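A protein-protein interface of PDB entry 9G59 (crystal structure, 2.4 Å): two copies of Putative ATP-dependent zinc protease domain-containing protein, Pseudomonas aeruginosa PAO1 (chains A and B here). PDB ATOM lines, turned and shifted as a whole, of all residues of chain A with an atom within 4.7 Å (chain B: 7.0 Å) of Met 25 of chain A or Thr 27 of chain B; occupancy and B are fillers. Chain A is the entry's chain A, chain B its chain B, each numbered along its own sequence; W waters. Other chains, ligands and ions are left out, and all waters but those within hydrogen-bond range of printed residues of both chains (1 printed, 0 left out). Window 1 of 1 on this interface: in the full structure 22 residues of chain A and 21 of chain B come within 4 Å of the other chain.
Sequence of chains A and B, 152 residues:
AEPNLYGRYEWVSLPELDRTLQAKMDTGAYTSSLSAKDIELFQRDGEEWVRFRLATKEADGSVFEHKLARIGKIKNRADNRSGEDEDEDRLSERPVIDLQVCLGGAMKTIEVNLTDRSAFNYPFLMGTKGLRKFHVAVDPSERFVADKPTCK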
ATOM      1  N   GLY A   7      -1.345  -1.948  -2.334  1.00  0.00           N
ATOM      2  CA  GLY A   7       0.036  -2.210  -1.996  1.00  0.00           C
ATOM      3  C   GLY A   7       0.522  -3.551  -2.513  1.00  0.00           C
ATOM      4  O   GLY A   7      -0.160  -4.259  -3.256  1.00  0.00           O
ATOM      5  N   ARG A   8       1.741  -3.900  -2.099  1.00  0.00           N
ATOM      6  CA  ARG A   8       2.328  -5.147  -2.569  1.00  0.00           C
ATOM      7  C   ARG A   8       1.679  -6.356  -1.909  1.00  0.00           C
ATOM      8  O   ARG A   8       1.709  -7.456  -2.471  1.00  0.00           O
ATOM      9  CB  ARG A   8       3.836  -5.148  -2.323  1.00  0.00           C
ATOM     10  CG  ARG A   8       4.575  -6.146  -3.185  1.00  0.00           C
ATOM     11  CD  ARG A   8       6.012  -6.304  -2.747  1.00  0.00           C
ATOM     12  NE  ARG A   8       6.722  -7.244  -3.604  1.00  0.00           N
ATOM     13  CZ  ARG A   8       7.914  -7.751  -3.328  1.00  0.00           C
ATOM     14  NH1 ARG A   8       8.548  -7.451  -2.206  1.00  0.00           N
ATOM     15  NH2 ARG A   8       8.482  -8.583  -4.196  1.00  0.00           N
ATOM     16  N   TYR A   9       1.090  -6.175  -0.730  1.00  0.00           N
ATOM     17  CA  TYR A   9       0.389  -7.236  -0.023  1.00  0.00           C
ATOM     18  C   TYR A   9      -0.942  -6.704   0.488  1.00  0.00           C
ATOM     19  O   TYR A   9      -1.008  -5.592   1.020  1.00  0.00           O
ATOM     20  CB  TYR A   9       1.212  -7.771   1.153  1.00  0.00           C
ATOM     21  CG  TYR A   9       2.706  -7.799   0.915  1.00  0.00           C
ATOM     22  CD1 TYR A   9       3.271  -8.696   0.019  1.00  0.00           C
ATOM     23  CD2 TYR A   9       3.550  -6.938   1.598  1.00  0.00           C
ATOM     24  CE1 TYR A   9       4.637  -8.727  -0.195  1.00  0.00           C
ATOM     25  CE2 TYR A   9       4.913  -6.960   1.393  1.00  0.00           C
ATOM     26  CZ  TYR A   9       5.451  -7.857   0.496  1.00  0.00           C
ATOM     27  OH  TYR A   9       6.809  -7.879   0.291  1.00  0.00           O
ATOM     28  N   GLU A  10      -1.995  -7.502   0.333  1.00  0.00           N
ATOM     29  CA  GLU A  10      -3.330  -7.096   0.757  1.00  0.00           C
ATOM     30  C   GLU A  10      -4.064  -8.273   1.382  1.00  0.00           C
ATOM     31  O   GLU A  10      -3.786  -9.436   1.086  1.00  0.00           O
ATOM     32  CB  GLU A  10      -4.162  -6.542  -0.410  1.00  0.00           C
ATOM     33  CG  GLU A  10      -3.630  -5.259  -1.018  1.00  0.00           C
ATOM     34  CD  GLU A  10      -3.749  -4.077  -0.079  1.00  0.00           C
ATOM     35  OE1 GLU A  10      -4.604  -4.122   0.831  1.00  0.00           O
ATOM     36  OE2 GLU A  10      -2.986  -3.105  -0.253  1.00  0.00           O
ATOM     37  N   ALA A  23      -2.317 -11.855   0.807  1.00  0.00           N
ATOM     38  CA  ALA A  23      -2.064 -12.121  -0.598  1.00  0.00           C
ATOM     39  C   ALA A  23      -0.981 -11.183  -1.100  1.00  0.00           C
ATOM     40  O   ALA A  23      -0.923 -10.015  -0.703  1.00  0.00           O
ATOM     41  CB  ALA A  23      -3.339 -11.949  -1.430  1.00  0.00           C
ATOM     42  N   LYS A  24      -0.119 -11.708  -1.965  1.00  0.00           N
ATOM     43  CA  LYS A  24       0.912 -10.915  -2.618  1.00  0.00           C
ATOM     44  C   LYS A  24       0.402 -10.490  -3.989  1.00  0.00           C
ATOM     45  O   LYS A  24      -0.021 -11.333  -4.786  1.00  0.00           O
ATOM     46  CB  LYS A  24       2.207 -11.713  -2.743  1.00  0.00           C
ATOM     47  CG  LYS A  24       3.338 -10.960  -3.419  1.00  0.00           C
ATOM     48  CD  LYS A  24       4.622 -11.768  -3.365  1.00  0.00           C
ATOM     49  CE  LYS A  24       5.796 -10.991  -3.926  1.00  0.00           C
ATOM     50  NZ  LYS A  24       7.076 -11.704  -3.666  1.00  0.00           N
ATOM     51  N   MET A  25       0.429  -9.187  -4.254  1.00  0.00           N
ATOM     52  CA  MET A  25      -0.071  -8.649  -5.516  1.00  0.00           C
ATOM     53  C   MET A  25       1.048  -8.730  -6.546  1.00  0.00           C
ATOM     54  O   MET A  25       2.015  -7.963  -6.484  1.00  0.00           O
ATOM     55  CB  MET A  25      -0.563  -7.218  -5.328  1.00  0.00           C
ATOM     56  CG  MET A  25      -1.585  -7.064  -4.216  1.00  0.00           C
ATOM     57  SD  MET A  25      -3.131  -7.944  -4.523  1.00  0.00           S
ATOM     58  CE  MET A  25      -3.329  -8.790  -2.966  1.00  0.00           C
ATOM     59  N   ASP A  26       0.915  -9.654  -7.496  1.00  0.00           N
ATOM     60  CA  ASP A  26       2.012 -10.071  -8.364  1.00  0.00           C
ATOM     61  C   ASP A  26       1.656  -9.752  -9.813  1.00  0.00           C
ATOM     62  O   ASP A  26       0.980 -10.539 -10.482  1.00  0.00           O
ATOM     63  CB  ASP A  26       2.287 -11.562  -8.171  1.00  0.00           C
ATOM     64  CG  ASP A  26       3.555 -12.024  -8.860  1.00  0.00           C
ATOM     65  OD1 ASP A  26       4.031 -11.323  -9.780  1.00  0.00           O
ATOM     66  OD2 ASP A  26       4.074 -13.095  -8.478  1.00  0.00           O
ATOM     67  N   THR A  27       2.138  -8.609 -10.309  1.00  0.00           N
ATOM     68  CA  THR A  27       1.943  -8.270 -11.714  1.00  0.00           C
ATOM     69  C   THR A  27       2.742  -9.157 -12.660  1.00  0.00           C
ATOM     70  O   THR A  27       2.486  -9.130 -13.868  1.00  0.00           O
ATOM     71  CB  THR A  27       2.309  -6.808 -11.978  1.00  0.00           C
ATOM     72  OG1 THR A  27       3.678  -6.581 -11.618  1.00  0.00           O
ATOM     73  CG2 THR A  27       1.409  -5.880 -11.178  1.00  0.00           C
ATOM     74  N   GLY A  28       3.696  -9.935 -12.152  1.00  0.00           N
ATOM     75  CA  GLY A  28       4.498 -10.793 -13.002  1.00  0.00           C
ATOM     76  C   GLY A  28       3.797 -12.092 -13.337  1.00  0.00           C
ATOM     77  O   GLY A  28       3.938 -12.623 -14.443  1.00  0.00           O
ATOM     78  N   MET A 126      -2.181 -13.055  -6.001  1.00  0.00           N
ATOM     79  CA  MET A 126      -3.095 -12.430  -6.950  1.00  0.00           C
ATOM     80  C   MET A 126      -2.319 -12.104  -8.222  1.00  0.00           C
ATOM     81  O   MET A 126      -1.482 -11.196  -8.234  1.00  0.00           O
ATOM     82  CB  MET A 126      -3.724 -11.180  -6.341  1.00  0.00           C
ATOM     83  CG  MET A 126      -4.634 -10.420  -7.285  1.00  0.00           C
ATOM     84  SD  MET A 126      -6.385 -10.754  -7.042  1.00  0.00           S
ATOM     85  CE  MET A 126      -6.613 -10.200  -5.353  1.00  0.00           C
ATOM     86  N   LEU A 131      -5.996  -9.115 -10.827  1.00  0.00           N
ATOM     87  CA  LEU A 131      -5.828  -7.678 -10.628  1.00  0.00           C
ATOM     88  C   LEU A 131      -6.650  -6.882 -11.635  1.00  0.00           C
ATOM     89  O   LEU A 131      -7.256  -5.863 -11.286  1.00  0.00           O
ATOM     90  CB  LEU A 131      -4.351  -7.304 -10.725  1.00  0.00           C
ATOM     91  CG  LEU A 131      -3.452  -7.843  -9.612  1.00  0.00           C
ATOM     92  CD1 LEU A 131      -1.985  -7.682  -9.979  1.00  0.00           C
ATOM     93  CD2 LEU A 131      -3.760  -7.143  -8.296  1.00  0.00           C
ATOM     94  N   VAL A 138      -0.854  -1.942  -8.560  1.00  0.00           N
ATOM     95  CA  VAL A 138      -0.020  -2.316  -7.423  1.00  0.00           C
ATOM     96  C   VAL A 138       1.089  -1.288  -7.243  1.00  0.00           C
ATOM     97  O   VAL A 138       1.942  -1.118  -8.121  1.00  0.00           O
ATOM     98  CB  VAL A 138       0.568  -3.723  -7.601  1.00  0.00           C
ATOM     99  CG1 VAL A 138       1.267  -4.162  -6.321  1.00  0.00           C
ATOM    100  CG2 VAL A 138      -0.518  -4.710  -7.993  1.00  0.00           C
ATOM    101  N   PRO A 140       4.302  -0.940  -5.361  1.00  0.00           N
ATOM    102  CA  PRO A 140       5.210  -1.798  -4.583  1.00  0.00           C
ATOM    103  C   PRO A 140       5.769  -1.133  -3.337  1.00  0.00           C
ATOM    104  O   PRO A 140       6.354  -1.832  -2.500  1.00  0.00           O
ATOM    105  CB  PRO A 140       6.329  -2.126  -5.582  1.00  0.00           C
ATOM    106  CG  PRO A 140       5.734  -1.847  -6.937  1.00  0.00           C
ATOM    107  CD  PRO A 140       4.794  -0.708  -6.728  1.00  0.00           C
ATOM    108  N   LYS B  24       9.095  -6.084 -18.591  1.00  0.00           N
ATOM    109  CA  LYS B  24       7.916  -6.496 -17.842  1.00  0.00           C
ATOM    110  C   LYS B  24       8.018  -5.937 -16.428  1.00  0.00           C
ATOM    111  O   LYS B  24       9.021  -6.156 -15.740  1.00  0.00           O
ATOM    112  CB  LYS B  24       7.805  -8.019 -17.821  1.00  0.00           C
ATOM    113  CG  LYS B  24       6.505  -8.551 -17.254  1.00  0.00           C
ATOM    114  CD  LYS B  24       6.479 -10.067 -17.344  1.00  0.00           C
ATOM    115  CE  LYS B  24       5.160 -10.636 -16.863  1.00  0.00           C
ATOM    116  NZ  LYS B  24       5.101 -12.107 -17.079  1.00  0.00           N
ATOM    117  N   MET B  25       6.988  -5.211 -16.000  1.00  0.00           N
ATOM    118  CA  MET B  25       6.976  -4.583 -14.682  1.00  0.00           C
ATOM    119  C   MET B  25       6.407  -5.578 -13.677  1.00  0.00           C
ATOM    120  O   MET B  25       5.198  -5.830 -13.658  1.00  0.00           O
ATOM    121  CB  MET B  25       6.165  -3.293 -14.726  1.00  0.00           C
ATOM    122  CG  MET B  25       6.480  -2.430 -15.942  1.00  0.00           C
ATOM    123  SD  MET B  25       8.208  -1.909 -16.021  1.00  0.00           S
ATOM    124  CE  MET B  25       8.117  -0.340 -15.169  1.00  0.00           C
ATOM    125  N   ASP B  26       7.277  -6.132 -12.834  1.00  0.00           N
ATOM    126  CA  ASP B  26       6.996  -7.338 -12.056  1.00  0.00           C
ATOM    127  C   ASP B  26       7.018  -6.999 -10.567  1.00  0.00           C
ATOM    128  O   ASP B  26       8.086  -6.951  -9.950  1.00  0.00           O
ATOM    129  CB  ASP B  26       8.020  -8.419 -12.396  1.00  0.00           C
ATOM    130  CG  ASP B  26       7.592  -9.801 -11.952  1.00  0.00           C
ATOM    131  OD1 ASP B  26       6.944  -9.919 -10.891  1.00  0.00           O
ATOM    132  OD2 ASP B  26       7.908 -10.772 -12.673  1.00  0.00           O
ATOM    133  N   THR B  27       5.833  -6.783  -9.988  1.00  0.00           N
ATOM    134  CA  THR B  27       5.717  -6.529  -8.557  1.00  0.00           C
ATOM    135  C   THR B  27       5.952  -7.772  -7.709  1.00  0.00           C
ATOM    136  O   THR B  27       6.117  -7.645  -6.491  1.00  0.00           O
ATOM    137  CB  THR B  27       4.337  -5.961  -8.218  1.00  0.00           C
ATOM    138  OG1 THR B  27       3.329  -6.895  -8.623  1.00  0.00           O
ATOM    139  CG2 THR B  27       4.117  -4.640  -8.927  1.00  0.00           C
ATOM    140  N   GLY B  28       5.960  -8.958  -8.307  1.00  0.00           N
ATOM    141  CA  GLY B  28       6.198 -10.172  -7.553  1.00  0.00           C
ATOM    142  C   GLY B  28       7.675 -10.404  -7.320  1.00  0.00           C
ATOM    143  O   GLY B  28       8.089 -10.801  -6.227  1.00  0.00           O
ATOM    144  N   ALA B  29       8.476 -10.150  -8.349  1.00  0.00           N
ATOM    145  CA  ALA B  29       9.918 -10.287  -8.235  1.00  0.00           C
ATOM    146  C   ALA B  29      10.490  -9.170  -7.366  1.00  0.00           C
ATOM    147  O   ALA B  29       9.882  -8.112  -7.185  1.00  0.00           O
ATOM    148  CB  ALA B  29      10.569 -10.263  -9.619  1.00  0.00           C
ATOM    149  N   TYR B  30      11.679  -9.420  -6.822  1.00  0.00           N
ATOM    150  CA  TYR B  30      12.400  -8.416  -6.047  1.00  0.00           C
ATOM    151  C   TYR B  30      13.556  -7.806  -6.835  1.00  0.00           C
ATOM    152  O   TYR B  30      13.621  -6.584  -6.992  1.00  0.00           O
ATOM    153  CB  TYR B  30      12.902  -9.030  -4.732  1.00  0.00           C
ATOM    154  CG  TYR B  30      13.611  -8.047  -3.823  1.00  0.00           C
ATOM    155  CD1 TYR B  30      12.896  -7.199  -2.989  1.00  0.00           C
ATOM    156  CD2 TYR B  30      14.999  -7.973  -3.798  1.00  0.00           C
ATOM    157  CE1 TYR B  30      13.543  -6.296  -2.156  1.00  0.00           C
ATOM    158  CE2 TYR B  30      15.654  -7.077  -2.971  1.00  0.00           C
ATOM    159  CZ  TYR B  30      14.924  -6.242  -2.152  1.00  0.00           C
ATOM    160  OH  TYR B  30      15.582  -5.353  -1.333  1.00  0.00           O
ATOM    161  N   MET B 126      11.860  -5.670 -14.620  1.00  0.00           N
ATOM    162  CA  MET B 126      12.087  -4.755 -13.509  1.00  0.00           C
ATOM    163  C   MET B 126      11.312  -5.258 -12.297  1.00  0.00           C
ATOM    164  O   MET B 126      10.076  -5.260 -12.297  1.00  0.00           O
ATOM    165  CB  MET B 126      11.678  -3.330 -13.868  1.00  0.00           C
ATOM    166  CG  MET B 126      12.144  -2.310 -12.846  1.00  0.00           C
ATOM    167  SD  MET B 126      11.952  -0.615 -13.415  1.00  0.00           S
ATOM    168  CE  MET B 126      13.034  -0.628 -14.843  1.00  0.00           C
ATOM    169  N   GLY B 127      12.043  -5.686 -11.272  1.00  0.00           N
ATOM    170  CA  GLY B 127      11.450  -6.158 -10.041  1.00  0.00           C
ATOM    171  C   GLY B 127      11.089  -5.020  -9.103  1.00  0.00           C
ATOM    172  O   GLY B 127      11.185  -3.837  -9.430  1.00  0.00           O
ATOM    173  N   THR B 128      10.682  -5.408  -7.892  1.00  0.00           N
ATOM    174  CA  THR B 128      10.108  -4.450  -6.953  1.00  0.00           C
ATOM    175  C   THR B 128      11.121  -3.387  -6.543  1.00  0.00           C
ATOM    176  O   THR B 128      10.762  -2.218  -6.354  1.00  0.00           O
ATOM    177  CB  THR B 128       9.566  -5.191  -5.728  1.00  0.00           C
ATOM    178  OG1 THR B 128       8.460  -6.016  -6.118  1.00  0.00           O
ATOM    179  CG2 THR B 128       9.108  -4.215  -4.666  1.00  0.00           C
ATOM    180  N   LEU B 131      11.299  -0.758  -9.253  1.00  0.00           N
ATOM    181  CA  LEU B 131      10.059   0.015  -9.280  1.00  0.00           C
ATOM    182  C   LEU B 131      10.004   1.009  -8.128  1.00  0.00           C
ATOM    183  O   LEU B 131       9.556   2.150  -8.302  1.00  0.00           O
ATOM    184  CB  LEU B 131       8.853  -0.922  -9.231  1.00  0.00           C
ATOM    185  CG  LEU B 131       8.708  -1.930 -10.371  1.00  0.00           C
ATOM    186  CD1 LEU B 131       7.646  -2.957 -10.024  1.00  0.00           C
ATOM    187  CD2 LEU B 131       8.368  -1.222 -11.672  1.00  0.00           C
ATOM    188  N   VAL B 136       7.397   3.784  -9.063  1.00  0.00           N
ATOM    189  CA  VAL B 136       6.461   3.369 -10.100  1.00  0.00           C
ATOM    190  C   VAL B 136       5.434   2.427  -9.491  1.00  0.00           C
ATOM    191  O   VAL B 136       5.778   1.563  -8.678  1.00  0.00           O
ATOM    192  CB  VAL B 136       7.202   2.694 -11.275  1.00  0.00           C
ATOM    193  CG1 VAL B 136       6.237   1.934 -12.171  1.00  0.00           C
ATOM    194  CG2 VAL B 136       7.969   3.729 -12.081  1.00  0.00           C
ATOM    195  N   ALA B 137       4.173   2.607  -9.872  1.00  0.00           N
ATOM    196  CA  ALA B 137       3.103   1.675  -9.554  1.00  0.00           C
ATOM    197  C   ALA B 137       2.589   1.080 -10.856  1.00  0.00           C
ATOM    198  O   ALA B 137       2.393   1.808 -11.835  1.00  0.00           O
ATOM    199  CB  ALA B 137       1.968   2.368  -8.795  1.00  0.00           C
ATOM    200  N   VAL B 138       2.352  -0.227 -10.859  1.00  0.00           N
ATOM    201  CA  VAL B 138       2.052  -0.968 -12.078  1.00  0.00           C
ATOM    202  C   VAL B 138       0.548  -1.172 -12.182  1.00  0.00           C
ATOM    203  O   VAL B 138      -0.067  -1.786 -11.302  1.00  0.00           O
ATOM    204  CB  VAL B 138       2.786  -2.316 -12.105  1.00  0.00           C
ATOM    205  CG1 VAL B 138       2.607  -2.987 -13.455  1.00  0.00           C
ATOM    206  CG2 VAL B 138       4.259  -2.126 -11.776  1.00  0.00           C
ATOM    207  N   PRO B 140      -1.790  -3.291 -14.246  1.00  0.00           N
ATOM    208  CA  PRO B 140      -1.741  -4.392 -15.225  1.00  0.00           C
ATOM    209  C   PRO B 140      -2.748  -4.263 -16.355  1.00  0.00           C
ATOM    210  O   PRO B 140      -2.652  -5.024 -17.327  1.00  0.00           O
ATOM    211  CB  PRO B 140      -2.031  -5.638 -14.375  1.00  0.00           C
ATOM    212  CG  PRO B 140      -1.789  -5.223 -12.961  1.00  0.00           C
ATOM    213  CD  PRO B 140      -2.141  -3.768 -12.899  1.00  0.00           C
HETATM  214  O   HOH W   1       7.293 -12.272 -14.645  1.00  0.00           O
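NH2 of Arg 8 of chain A sits at hydrogen-bond distance from O of Gly 28 of chain B, 3.0 Å away. N of Thr 27 of chain A is in hydrogen-bond range of OG1 of Thr 27 of chain B (2.7 Å). O of Gly 28 of chain A lies within hydrogen-bond range of NZ of Lys 24 of chain B (2.9 Å). OG1 of Thr 27 of chain B lies within hydrogen-bond range of O of Met 25 of chain A, at 2.7 Å. The guanidinium group (NE) of Arg 8 of chain A lies within hydrogen-bond range of the backbone carbonyl oxygen (O) of Thr 27 of chain B (3.0 Å). The backbone NH (N) of Gly 28 of chain A lies close to the side-chain carboxylate (OD1) of Asp 26 of chain B (3.5 Å). N of Val 138 of chain A sits at hydrogen-bond distance from O of Val 138 of chain B. N of Gly 28 of chain B lies close to OD1 of Asp 26 of chain A (3.4 Å). The side-chain hydroxyl of Thr 27 of chain A sits at hydrogen-bond distance from the backbone carbonyl oxygen of Met 25 of chain B, at 2.7 Å. The guanidinium group (NH2) of Arg 8 of chain A is in hydrogen-bond range of the backbone carbonyl oxygen (O) of Ala 29 of chain B, 3.3 Å away. NZ of Lys 24 of chain A lies within hydrogen-bond range of O of Gly 28 of chain B, 2.9 Å away. The side-chain carboxylate (OD1) of Asp 26 of chain A sits close to the side-chain carboxylate (OD1) of Asp 26 of chain B (3.4 Å). The guanidinium group of Arg 8 of chain A lies within hydrogen-bond range of the side-chain hydroxyl of Thr 128 of chain B.
The backbone carbonyl oxygen of Lys 24 of chain B is in hydrogen-bond range of the backbone NH of Met 126 of chain B. OG1 of Thr 128 of chain B sits at hydrogen-bond distance from O of Thr 27 of chain B. The backbone carbonyl oxygen of Met 126 of chain B sits at hydrogen-bond distance from the backbone NH of Asp 26 of chain B (3.0 Å). OD1 of Asp 26 of chain B lies within hydrogen-bond range of N of Ala 29 of chain B (3.0 Å). The side-chain carboxylate (OD1) of Asp 26 of chain B lies within hydrogen-bond range of the backbone NH (N) of Gly 28 of chain B (2.9 Å). The backbone carbonyl oxygen (O) of Arg 8 of chain A lies within hydrogen-bond range of the backbone NH (N) of Met 25 of chain A, 2.8 Å away.
Among the printed residues, merely in contact across the chains: Asp 26 of chain A with Thr 27 of chain B (3.4 Å), Thr 27 of chain A with Asp 26 of chain B (3.4 Å), Thr 27 of chain A with Val 138 of chain B (3.9 Å), Thr 27 of chain A with Pro 140 of chain B (3.7 Å), Leu 131 of chain A with Pro 140 of chain B (3.9 Å), Val 138 of chain A with Thr 27 of chain B (3.9 Å), Val 138 of chain A with Ala 137 of chain B (3.3 Å), Pro 140 of chain A with Thr 27 of chain B (3.8 Å), Pro 140 of chain A with Thr 128 of chain B (3.6 Å), Pro 140 of chain A with Leu 131 of chain B (3.8 Å) and Pro 140 of chain A with Val 136 of chain B (3.2 Å).
Of chain A, only Arg 8, Met 25, Asp 26, Thr 27, Val 138 and Pro 140 come within 4 Å of Thr 27 of chain B. Printed residues of chain B within 4 Å of Gly 28 of chain A: Lys 24 (2.9 Å) and Asp 26 (3.3 Å). Printed residues of chain A within 4 Å of Ala 29 of chain B: Arg 8. Of the printed residues of chain A, Ala 137 of chain B touches Val 138. Tyr 9 of chain A touches none of the printed residues of chain B. The nearest residue of chain A that does not touch Thr 27 of chain B is Lys 24 of chain A (4.2 Å). The nearest printed residue of chain A that does not touch Lys 24 of chain B is Thr 27 of chain A (4.3 Å).
Printed residues of chain B that touch a printed residue of chain A: Lys 24, Met 25, Asp 26, Thr 27, Gly 28, Ala 29, Thr 128, Leu 131, Val 136, Ala 137, Val 138 and Pro 140. Hydrophobic or aromatic side chains of chain B within 4 Å of the printed part of chain A: Leu 131, Ala 137, Val 138 and Pro 140. Hydrophobic or aromatic side chains of chain A that line the printed part of chain B: Leu 131, Val 138 and Pro 140. Along chain A the printed residues that touch a printed residue of chain B span positions 8 to 140. Among the printed residues, 24 pairs touch across the chains. Among the printed residues, no Asp or Glu carboxylate lies within 4 Å of a Lys or Arg side-chain nitrogen of the other chain.
Met 25 of chain A touches Thr 27 of chain B, and with the chains exchanged Thr 27 of chain A touches Met 25 of chain B. Asp 26 of chain B touches its own counterpart, Asp 26 of chain A. Thr 27 of chain B touches its own counterpart, Thr 27 of chain A. Thr 27 of chain A touches Pro 140 of chain B, and with the chains exchanged Pro 140 of chain A touches Thr 27 of chain B.
Water W1 lies within hydrogen-bond range of the side-chain carboxylate (OD2) of Asp 26 of chain B (2.6 Å), the side-chain amino group (NZ) of Lys 24 of chain B (3.3 Å) and the backbone carbonyl oxygen (O) of Gly 28 of chain A (3.4 Å).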
